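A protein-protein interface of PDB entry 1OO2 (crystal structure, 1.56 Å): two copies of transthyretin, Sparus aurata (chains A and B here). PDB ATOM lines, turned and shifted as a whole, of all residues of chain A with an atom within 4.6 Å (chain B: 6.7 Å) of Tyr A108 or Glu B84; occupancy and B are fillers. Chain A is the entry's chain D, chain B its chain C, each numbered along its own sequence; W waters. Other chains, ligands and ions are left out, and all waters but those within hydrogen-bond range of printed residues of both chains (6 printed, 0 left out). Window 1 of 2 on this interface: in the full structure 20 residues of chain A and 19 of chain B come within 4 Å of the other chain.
Glu A84 touches Tyr B108, and with the chains exchanged Tyr A108 touches Glu B84. Val A86 touches Val B82, but with the chains exchanged Val A82 does not touch Val B86 (4.3 Å). Tyr A108 touches Thr B109, and with the chains exchanged Thr A109 touches Tyr B108. Thr B109 touches its own counterpart, Thr A109. Positions printed for both chains: 62, 82, 83, 84, 86, 108, 109 and 110.
Along chain B the printed residues that touch a printed residue of chain A span positions 82 to 111. Printed residues of chain A that touch a printed residue of chain B: Arg A62, His A80, Glu A84, Val A86, Ser A107, Tyr A108, Thr A109 and Thr A110. Hydrophobic or aromatic side chains of chain A within 4 Å of the printed part of chain B: His A80, Val A86 and Tyr A108. Among the printed residues, Asp or Glu carboxylates within 4 Å of a Lys or Arg side-chain nitrogen of the other chain: Arg A62 with Glu B84 (2.9 Å).
Among the printed residues, merely in contact across the chains: His A80 with Val B86 (3.3 Å), Tyr A108 with Thr B109 (3.4 Å), Val A86 with Glu B84 (3.5 Å), Thr A109 with Tyr B108 (3.5 Å), Glu A84 with Glu B84 (3.6 Å), Glu A84 with Val B86 (3.7 Å), Ser A107 with Thr B109 (3.9 Å), Val A86 with Val B82 (3.9 Å) and His A80 with Val B85 (3.95 Å).
The backbone carbonyl oxygen (O) of Val B63 sits at hydrogen-bond distance from the backbone NH (N) of Val B85 (2.9 Å). The guanidinium group of Arg A62 lies within salt-bridge range of the side-chain carboxylate of Glu A84 (3.8 Å). The backbone carbonyl oxygen (O) of Thr A109 lies within hydrogen-bond range of the backbone NH (N) of Leu A102, at 2.8 Å.
Of the printed residues of chain B, His A80 touches Val B85 (3.95 Å), Val B86 (3.3 Å) and Thr B110 (3.1 Å). Of the printed residues of chain B, Val A86 touches Val B82 and Glu B84. Leu A101 touches none of the printed residues of chain B. Printed residues of chain B within 4 Å of Tyr A108: Glu B84 (3.4 Å), Thr B109 (3.4 Å) and Thr B110 (2.9 Å). Glu B64 touches none of the printed residues of chain A. Of the printed residues of chain A, Glu B84 touches Arg A62 (2.9 Å), Glu A84 (3.6 Å), Val A86 (3.5 Å) and Tyr A108 (3.4 Å). Of the printed residues of chain A, Thr B109 touches Ser A107 (3.9 Å), Tyr A108 (3.4 Å) and Thr A109 (2.7 Å). The nearest printed residue of chain A that does not touch Tyr B108 is Tyr A108 (4.01 Å).
Water W4 bridges OE1 of Glu A84 (2.5 Å) and O of Glu B84 (3.1 Å). Water W5 lies within hydrogen-bond range of the side-chain carboxylate of Glu A84 (2.6 Å), the guanidinium group of Arg A62 (2.8 Å) and the guanidinium group of Arg B62 (3.1 Å). Water W6 lies within hydrogen-bond range of the side-chain hydroxyl of Tyr A108 (2.6 Å), the side-chain hydroxyl of Tyr B108 (2.7 Å), the backbone carbonyl oxygen of Glu B84 (2.7 Å) and the backbone carbonyl oxygen of Glu A84 (2.8 Å). Water W3 lies within hydrogen-bond range of O of Val B82 (2.7 Å), OH of Tyr B108 (2.8 Å) and N of Val A86 (3.0 Å). Water W2 lies within hydrogen-bond range of the backbone carbonyl oxygen (O) of Val A82 (2.8 Å), the side-chain hydroxyl (OH) of Tyr A108 (2.8 Å), the backbone NH (N) of Val B86 (2.9 Å) and the backbone carbonyl oxygen (O) of Glu B84 (3.4 Å). Water W1 lies within hydrogen-bond range of N of Glu B84 (2.9 Å) and O of Glu A84 (2.9 Å).
The side-chain carboxylate (OE1) of Glu B84 lies within salt-bridge range of the guanidinium group (NH2) of Arg A62 (2.9 Å). The backbone carbonyl oxygen of Glu B84 lies within hydrogen-bond range of the side-chain hydroxyl of Tyr A108. OH of Tyr B108 lies within hydrogen-bond range of O of Glu A84 (3.4 Å). The backbone carbonyl oxygen of Tyr B108 is in hydrogen-bond range of the backbone NH of Thr A110, at 2.9 Å. The side-chain hydroxyl (OG1) of Thr B109 sits at hydrogen-bond distance from the side-chain hydroxyl (OG1) of Thr A109, at 2.7 Å. The side-chain hydroxyl of Thr B110 sits at hydrogen-bond distance from a ring nitrogen (NE2) of His A80 (3.1 Å). The side-chain hydroxyl (OG) of Ser A107 sits at hydrogen-bond distance from the backbone carbonyl oxygen (O) of Thr B110 (3.0 Å). The backbone carbonyl oxygen (O) of Tyr A108 is in hydrogen-bond range of the backbone NH (N) of Thr B110 (2.9 Å). The side-chain hydroxyl of Thr B111 sits at hydrogen-bond distance from the side-chain hydroxyl of Ser A107, 2.8 Å away.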
ATOM      1  N   ARG A  62       6.949  23.234 -16.762  1.00  0.00           N
ATOM      2  CA  ARG A  62       5.926  22.775 -15.823  1.00  0.00           C
ATOM      3  C   ARG A  62       6.021  21.266 -15.699  1.00  0.00           C
ATOM      4  O   ARG A  62       5.951  20.527 -16.684  1.00  0.00           O
ATOM      5  CB  ARG A  62       4.549  23.242 -16.285  1.00  0.00           C
ATOM      6  CG  ARG A  62       3.341  22.684 -15.562  1.00  0.00           C
ATOM      7  CD  ARG A  62       2.045  23.199 -16.194  1.00  0.00           C
ATOM      8  NE  ARG A  62       1.885  24.638 -15.996  1.00  0.00           N
ATOM      9  CZ  ARG A  62       1.325  25.202 -14.932  1.00  0.00           C
ATOM     10  NH1 ARG A  62       1.238  26.522 -14.852  1.00  0.00           N
ATOM     11  NH2 ARG A  62       0.857  24.446 -13.948  1.00  0.00           N
ATOM     12  N   HIS A  80      -5.171  17.001  -2.822  1.00  0.00           N
ATOM     13  CA  HIS A  80      -4.818  17.690  -4.065  1.00  0.00           C
ATOM     14  C   HIS A  80      -5.197  16.893  -5.305  1.00  0.00           C
ATOM     15  O   HIS A  80      -5.113  15.665  -5.347  1.00  0.00           O
ATOM     16  CB  HIS A  80      -3.317  17.951  -4.124  1.00  0.00           C
ATOM     17  CG  HIS A  80      -2.750  18.782  -3.022  1.00  0.00           C
ATOM     18  ND1 HIS A  80      -2.313  18.258  -1.824  1.00  0.00           N
ATOM     19  CD2 HIS A  80      -2.491  20.113  -2.965  1.00  0.00           C
ATOM     20  CE1 HIS A  80      -1.831  19.228  -1.061  1.00  0.00           C
ATOM     21  NE2 HIS A  80      -1.938  20.369  -1.733  1.00  0.00           N
ATOM     22  N   VAL A  82      -3.502  17.311  -8.181  1.00  0.00           N
ATOM     23  CA  VAL A  82      -2.207  17.171  -8.810  1.00  0.00           C
ATOM     24  C   VAL A  82      -1.186  17.993  -8.018  1.00  0.00           C
ATOM     25  O   VAL A  82      -1.600  18.828  -7.202  1.00  0.00           O
ATOM     26  CB  VAL A  82      -2.149  17.668 -10.271  1.00  0.00           C
ATOM     27  CG1 VAL A  82      -2.968  16.811 -11.214  1.00  0.00           C
ATOM     28  CG2 VAL A  82      -2.596  19.124 -10.345  1.00  0.00           C
ATOM     29  N   ALA A  83       0.093  17.757  -8.253  1.00  0.00           N
ATOM     30  CA  ALA A  83       1.145  18.645  -7.782  1.00  0.00           C
ATOM     31  C   ALA A  83       1.872  19.189  -9.012  1.00  0.00           C
ATOM     32  O   ALA A  83       2.425  18.409  -9.792  1.00  0.00           O
ATOM     33  CB  ALA A  83       2.148  17.974  -6.867  1.00  0.00           C
ATOM     34  N   GLU A  84       1.858  20.499  -9.203  1.00  0.00           N
ATOM     35  CA  GLU A  84       2.553  21.101 -10.331  1.00  0.00           C
ATOM     36  C   GLU A  84       3.742  21.915  -9.832  1.00  0.00           C
ATOM     37  O   GLU A  84       3.641  22.644  -8.843  1.00  0.00           O
ATOM     38  CB  GLU A  84       1.616  22.039 -11.097  1.00  0.00           C
ATOM     39  CG  GLU A  84       0.518  21.335 -11.875  1.00  0.00           C
ATOM     40  CD  GLU A  84      -0.813  22.061 -11.865  1.00  0.00           C
ATOM     41  OE1 GLU A  84      -1.047  22.956 -11.022  1.00  0.00           O
ATOM     42  OE2 GLU A  84      -1.663  21.728 -12.726  1.00  0.00           O
ATOM     43  N   VAL A  86       6.478  24.688 -11.309  1.00  0.00           N
ATOM     44  CA  VAL A  86       6.734  25.582 -12.428  1.00  0.00           C
ATOM     45  C   VAL A  86       7.977  26.425 -12.199  1.00  0.00           C
ATOM     46  O   VAL A  86       8.087  27.052 -11.136  1.00  0.00           O
ATOM     47  CB  VAL A  86       5.533  26.533 -12.633  1.00  0.00           C
ATOM     48  CG1 VAL A  86       5.691  27.331 -13.921  1.00  0.00           C
ATOM     49  CG2 VAL A  86       4.245  25.731 -12.639  1.00  0.00           C
ATOM     50  N   LEU A 101      10.208  15.872  -4.022  1.00  0.00           N
ATOM     51  CA  LEU A 101       8.776  15.971  -3.750  1.00  0.00           C
ATOM     52  C   LEU A 101       8.436  14.982  -2.643  1.00  0.00           C
ATOM     53  O   LEU A 101       8.691  13.789  -2.815  1.00  0.00           O
ATOM     54  CB  LEU A 101       7.968  15.630  -5.000  1.00  0.00           C
ATOM     55  CG  LEU A 101       6.793  16.431  -5.516  1.00  0.00           C
ATOM     56  CD1 LEU A 101       5.840  15.513  -6.295  1.00  0.00           C
ATOM     57  CD2 LEU A 101       6.048  17.192  -4.431  1.00  0.00           C
ATOM     58  N   LEU A 102       7.926  15.469  -1.522  1.00  0.00           N
ATOM     59  CA  LEU A 102       7.562  14.580  -0.417  1.00  0.00           C
ATOM     60  C   LEU A 102       6.048  14.576  -0.260  1.00  0.00           C
ATOM     61  O   LEU A 102       5.478  15.650  -0.056  1.00  0.00           O
ATOM     62  CB  LEU A 102       8.215  15.037   0.886  1.00  0.00           C
ATOM     63  CG  LEU A 102       7.888  14.294   2.167  1.00  0.00           C
ATOM     64  CD1 LEU A 102       8.500  12.901   2.182  1.00  0.00           C
ATOM     65  CD2 LEU A 102       8.379  15.095   3.373  1.00  0.00           C
ATOM     66  N   LEU A 103       5.424  13.417  -0.369  1.00  0.00           N
ATOM     67  CA  LEU A 103       3.965  13.315  -0.454  1.00  0.00           C
ATOM     68  C   LEU A 103       3.308  12.787   0.819  1.00  0.00           C
ATOM     69  O   LEU A 103       3.779  11.787   1.358  1.00  0.00           O
ATOM     70  CB  LEU A 103       3.553  12.376  -1.605  1.00  0.00           C
ATOM     71  CG  LEU A 103       4.124  12.725  -2.986  1.00  0.00           C
ATOM     72  CD1 LEU A 103       3.595  11.720  -4.008  1.00  0.00           C
ATOM     73  CD2 LEU A 103       3.751  14.144  -3.370  1.00  0.00           C
ATOM     74  N   SER A 107      -0.858  16.866   2.146  1.00  0.00           N
ATOM     75  CA  SER A 107       0.252  17.818   2.089  1.00  0.00           C
ATOM     76  C   SER A 107       1.311  17.342   1.113  1.00  0.00           C
ATOM     77  O   SER A 107       1.529  16.137   0.985  1.00  0.00           O
ATOM     78  CB  SER A 107       0.846  17.969   3.498  1.00  0.00           C
ATOM     79  OG  SER A 107       1.949  18.865   3.520  1.00  0.00           O
ATOM     80  N   TYR A 108       2.001  18.262   0.428  1.00  0.00           N
ATOM     81  CA  TYR A 108       3.292  17.919  -0.158  1.00  0.00           C
ATOM     82  C   TYR A 108       4.299  19.036   0.099  1.00  0.00           C
ATOM     83  O   TYR A 108       3.948  20.215   0.180  1.00  0.00           O
ATOM     84  CB  TYR A 108       3.247  17.602  -1.648  1.00  0.00           C
ATOM     85  CG  TYR A 108       2.657  18.624  -2.582  1.00  0.00           C
ATOM     86  CD1 TYR A 108       3.442  19.609  -3.184  1.00  0.00           C
ATOM     87  CD2 TYR A 108       1.297  18.581  -2.871  1.00  0.00           C
ATOM     88  CE1 TYR A 108       2.873  20.538  -4.044  1.00  0.00           C
ATOM     89  CE2 TYR A 108       0.728  19.508  -3.731  1.00  0.00           C
ATOM     90  CZ  TYR A 108       1.526  20.472  -4.314  1.00  0.00           C
ATOM     91  OH  TYR A 108       0.946  21.398  -5.164  1.00  0.00           O
ATOM     92  N   THR A 109       5.554  18.625   0.187  1.00  0.00           N
ATOM     93  CA  THR A 109       6.703  19.528   0.215  1.00  0.00           C
ATOM     94  C   THR A 109       7.505  19.370  -1.064  1.00  0.00           C
ATOM     95  O   THR A 109       7.844  18.248  -1.466  1.00  0.00           O
ATOM     96  CB  THR A 109       7.607  19.203   1.407  1.00  0.00           C
ATOM     97  OG1 THR A 109       6.869  19.402   2.623  1.00  0.00           O
ATOM     98  CG2 THR A 109       8.828  20.120   1.442  1.00  0.00           C
ATOM     99  N   THR A 110       7.820  20.476  -1.724  1.00  0.00           N
ATOM    100  CA  THR A 110       8.671  20.329  -2.906  1.00  0.00           C
ATOM    101  C   THR A 110       9.835  21.308  -2.840  1.00  0.00           C
ATOM    102  O   THR A 110       9.695  22.417  -2.332  1.00  0.00           O
ATOM    103  CB  THR A 110       7.891  20.492  -4.214  1.00  0.00           C
ATOM    104  OG1 THR A 110       8.782  20.181  -5.297  1.00  0.00           O
ATOM    105  CG2 THR A 110       7.374  21.899  -4.441  1.00  0.00           C
ATOM    106  N   ARG B  62      -8.500  26.097  -7.894  1.00  0.00           N
ATOM    107  CA  ARG B  62      -7.067  26.359  -8.009  1.00  0.00           C
ATOM    108  C   ARG B  62      -6.760  27.683  -7.312  1.00  0.00           C
ATOM    109  O   ARG B  62      -7.420  28.688  -7.560  1.00  0.00           O
ATOM    110  CB  ARG B  62      -6.621  26.435  -9.460  1.00  0.00           C
ATOM    111  CG  ARG B  62      -5.101  26.576  -9.555  1.00  0.00           C
ATOM    112  CD  ARG B  62      -4.703  27.697 -10.490  1.00  0.00           C
ATOM    113  NE  ARG B  62      -5.465  27.635 -11.738  1.00  0.00           N
ATOM    114  CZ  ARG B  62      -5.177  26.711 -12.652  1.00  0.00           C
ATOM    115  NH1 ARG B  62      -5.853  26.637 -13.784  1.00  0.00           N
ATOM    116  NH2 ARG B  62      -4.194  25.849 -12.417  1.00  0.00           N
ATOM    117  N   VAL B  63      -5.774  27.694  -6.419  1.00  0.00           N
ATOM    118  CA  VAL B  63      -5.249  28.961  -5.917  1.00  0.00           C
ATOM    119  C   VAL B  63      -3.827  29.142  -6.427  1.00  0.00           C
ATOM    120  O   VAL B  63      -2.975  28.279  -6.183  1.00  0.00           O
ATOM    121  CB  VAL B  63      -5.245  28.994  -4.374  1.00  0.00           C
ATOM    122  CG1 VAL B  63      -4.744  30.358  -3.915  1.00  0.00           C
ATOM    123  CG2 VAL B  63      -6.637  28.674  -3.859  1.00  0.00           C
ATOM    124  N   GLU B  64      -3.586  30.240  -7.137  1.00  0.00           N
ATOM    125  CA  GLU B  64      -2.268  30.572  -7.669  1.00  0.00           C
ATOM    126  C   GLU B  64      -1.651  31.618  -6.755  1.00  0.00           C
ATOM    127  O   GLU B  64      -2.160  32.735  -6.667  1.00  0.00           O
ATOM    128  CB  GLU B  64      -2.419  31.093  -9.092  1.00  0.00           C
ATOM    129  CG  GLU B  64      -1.242  31.824  -9.697  1.00  0.00           C
ATOM    130  CD  GLU B  64      -1.679  32.568 -10.957  1.00  0.00           C
ATOM    131  OE1 GLU B  64      -2.589  32.024 -11.627  1.00  0.00           O
ATOM    132  OE2 GLU B  64      -1.109  33.651 -11.207  1.00  0.00           O
ATOM    133  N   PHE B  65      -0.603  31.228  -6.031  1.00  0.00           N
ATOM    134  CA  PHE B  65       0.033  32.163  -5.107  1.00  0.00           C
ATOM    135  C   PHE B  65       1.260  32.771  -5.785  1.00  0.00           C
ATOM    136  O   PHE B  65       2.069  32.030  -6.353  1.00  0.00           O
ATOM    137  CB  PHE B  65       0.467  31.441  -3.839  1.00  0.00           C
ATOM    138  CG  PHE B  65      -0.602  30.809  -2.979  1.00  0.00           C
ATOM    139  CD1 PHE B  65      -1.132  31.519  -1.912  1.00  0.00           C
ATOM    140  CD2 PHE B  65      -1.046  29.516  -3.193  1.00  0.00           C
ATOM    141  CE1 PHE B  65      -2.076  30.968  -1.074  1.00  0.00           C
ATOM    142  CE2 PHE B  65      -2.014  28.958  -2.359  1.00  0.00           C
ATOM    143  CZ  PHE B  65      -2.513  29.670  -1.276  1.00  0.00           C
ATOM    144  N   VAL B  82       5.651  30.316  -9.642  1.00  0.00           N
ATOM    145  CA  VAL B  82       4.381  30.420  -8.958  1.00  0.00           C
ATOM    146  C   VAL B  82       4.263  29.212  -8.021  1.00  0.00           C
ATOM    147  O   VAL B  82       5.032  28.268  -8.215  1.00  0.00           O
ATOM    148  CB  VAL B  82       3.169  30.375  -9.918  1.00  0.00           C
ATOM    149  CG1 VAL B  82       3.016  31.636 -10.742  1.00  0.00           C
ATOM    150  CG2 VAL B  82       3.278  29.132 -10.786  1.00  0.00           C
ATOM    151  N   ALA B  83       3.321  29.240  -7.088  1.00  0.00           N
ATOM    152  CA  ALA B  83       2.917  28.061  -6.356  1.00  0.00           C
ATOM    153  C   ALA B  83       1.411  27.864  -6.505  1.00  0.00           C
ATOM    154  O   ALA B  83       0.633  28.671  -5.987  1.00  0.00           O
ATOM    155  CB  ALA B  83       3.290  28.150  -4.891  1.00  0.00           C
ATOM    156  N   GLU B  84       1.072  26.812  -7.245  1.00  0.00           N
ATOM    157  CA  GLU B  84      -0.322  26.499  -7.520  1.00  0.00           C
ATOM    158  C   GLU B  84      -0.809  25.372  -6.612  1.00  0.00           C
ATOM    159  O   GLU B  84      -0.118  24.378  -6.410  1.00  0.00           O
ATOM    160  CB  GLU B  84      -0.488  26.079  -8.991  1.00  0.00           C
ATOM    161  CG  GLU B  84      -0.225  27.250  -9.931  1.00  0.00           C
ATOM    162  CD  GLU B  84       0.215  26.848 -11.320  1.00  0.00           C
ATOM    163  OE1 GLU B  84       0.990  25.879 -11.462  1.00  0.00           O
ATOM    164  OE2 GLU B  84      -0.208  27.527 -12.282  1.00  0.00           O
ATOM    165  N   VAL B  85      -1.996  25.553  -6.047  1.00  0.00           N
ATOM    166  CA  VAL B  85      -2.573  24.524  -5.189  1.00  0.00           C
ATOM    167  C   VAL B  85      -3.944  24.170  -5.767  1.00  0.00           C
ATOM    168  O   VAL B  85      -4.842  25.012  -5.815  1.00  0.00           O
ATOM    169  CB  VAL B  85      -2.703  25.009  -3.745  1.00  0.00           C
ATOM    170  CG1 VAL B  85      -3.401  23.958  -2.888  1.00  0.00           C
ATOM    171  CG2 VAL B  85      -1.347  25.378  -3.146  1.00  0.00           C
ATOM    172  N   VAL B  86      -4.093  22.937  -6.243  1.00  0.00           N
ATOM    173  CA  VAL B  86      -5.310  22.523  -6.938  1.00  0.00           C
ATOM    174  C   VAL B  86      -5.973  21.420  -6.132  1.00  0.00           C
ATOM    175  O   VAL B  86      -5.334  20.412  -5.805  1.00  0.00           O
ATOM    176  CB  VAL B  86      -4.988  22.030  -8.360  1.00  0.00           C
ATOM    177  CG1 VAL B  86      -6.244  21.600  -9.103  1.00  0.00           C
ATOM    178  CG2 VAL B  86      -4.271  23.124  -9.152  1.00  0.00           C
ATOM    179  N   TYR B 108       8.634  24.895  -1.110  1.00  0.00           N
ATOM    180  CA  TYR B 108       7.444  25.233  -0.332  1.00  0.00           C
ATOM    181  C   TYR B 108       6.730  23.964   0.127  1.00  0.00           C
ATOM    182  O   TYR B 108       6.806  22.930  -0.533  1.00  0.00           O
ATOM    183  CB  TYR B 108       6.499  26.178  -1.069  1.00  0.00           C
ATOM    184  CG  TYR B 108       6.015  25.727  -2.428  1.00  0.00           C
ATOM    185  CD1 TYR B 108       4.844  24.994  -2.580  1.00  0.00           C
ATOM    186  CD2 TYR B 108       6.726  26.054  -3.576  1.00  0.00           C
ATOM    187  CE1 TYR B 108       4.396  24.584  -3.832  1.00  0.00           C
ATOM    188  CE2 TYR B 108       6.298  25.656  -4.835  1.00  0.00           C
ATOM    189  CZ  TYR B 108       5.134  24.923  -4.949  1.00  0.00           C
ATOM    190  OH  TYR B 108       4.696  24.523  -6.197  1.00  0.00           O
ATOM    191  N   THR B 109       6.040  24.071   1.252  1.00  0.00           N
ATOM    192  CA  THR B 109       5.126  23.037   1.758  1.00  0.00           C
ATOM    193  C   THR B 109       3.685  23.537   1.693  1.00  0.00           C
ATOM    194  O   THR B 109       3.424  24.660   2.151  1.00  0.00           O
ATOM    195  CB  THR B 109       5.554  22.678   3.190  1.00  0.00           C
ATOM    196  OG1 THR B 109       6.828  22.024   3.165  1.00  0.00           O
ATOM    197  CG2 THR B 109       4.585  21.715   3.868  1.00  0.00           C
ATOM    198  N   THR B 110       2.784  22.749   1.114  1.00  0.00           N
ATOM    199  CA  THR B 110       1.356  23.052   1.007  1.00  0.00           C
ATOM    200  C   THR B 110       0.587  21.989   1.786  1.00  0.00           C
ATOM    201  O   THR B 110       0.757  20.791   1.526  1.00  0.00           O
ATOM    202  CB  THR B 110       0.808  23.148  -0.426  1.00  0.00           C
ATOM    203  OG1 THR B 110      -0.629  22.928  -0.512  1.00  0.00           O
ATOM    204  CG2 THR B 110       1.369  22.102  -1.381  1.00  0.00           C
ATOM    205  N   THR B 111      -0.242  22.416   2.725  1.00  0.00           N
ATOM    206  CA  THR B 111      -1.122  21.489   3.409  1.00  0.00           C
ATOM    207  C   THR B 111      -2.526  22.086   3.493  1.00  0.00           C
ATOM    208  O   THR B 111      -2.704  23.244   3.122  1.00  0.00           O
ATOM    209  CB  THR B 111      -0.644  21.157   4.839  1.00  0.00           C
ATOM    210  OG1 THR B 111       0.787  21.012   4.821  1.00  0.00           O
ATOM    211  CG2 THR B 111      -1.254  19.835   5.260  1.00  0.00           C
HETATM  212  O   HOH W   1       2.782  25.432  -9.169  1.00  0.00           O
HETATM  213  O   HOH W   2      -1.703  21.354  -6.049  1.00  0.00           O
HETATM  214  O   HOH W   3       5.657  25.626  -8.619  1.00  0.00           O
HETATM  215  O   HOH W   4      -0.317  22.225  -8.696  1.00  0.00           O
HETATM  216  O   HOH W   5      -1.943  24.137 -13.665  1.00  0.00           O
HETATM  217  O   HOH W   6       2.336  23.212  -6.469  1.00  0.00           O
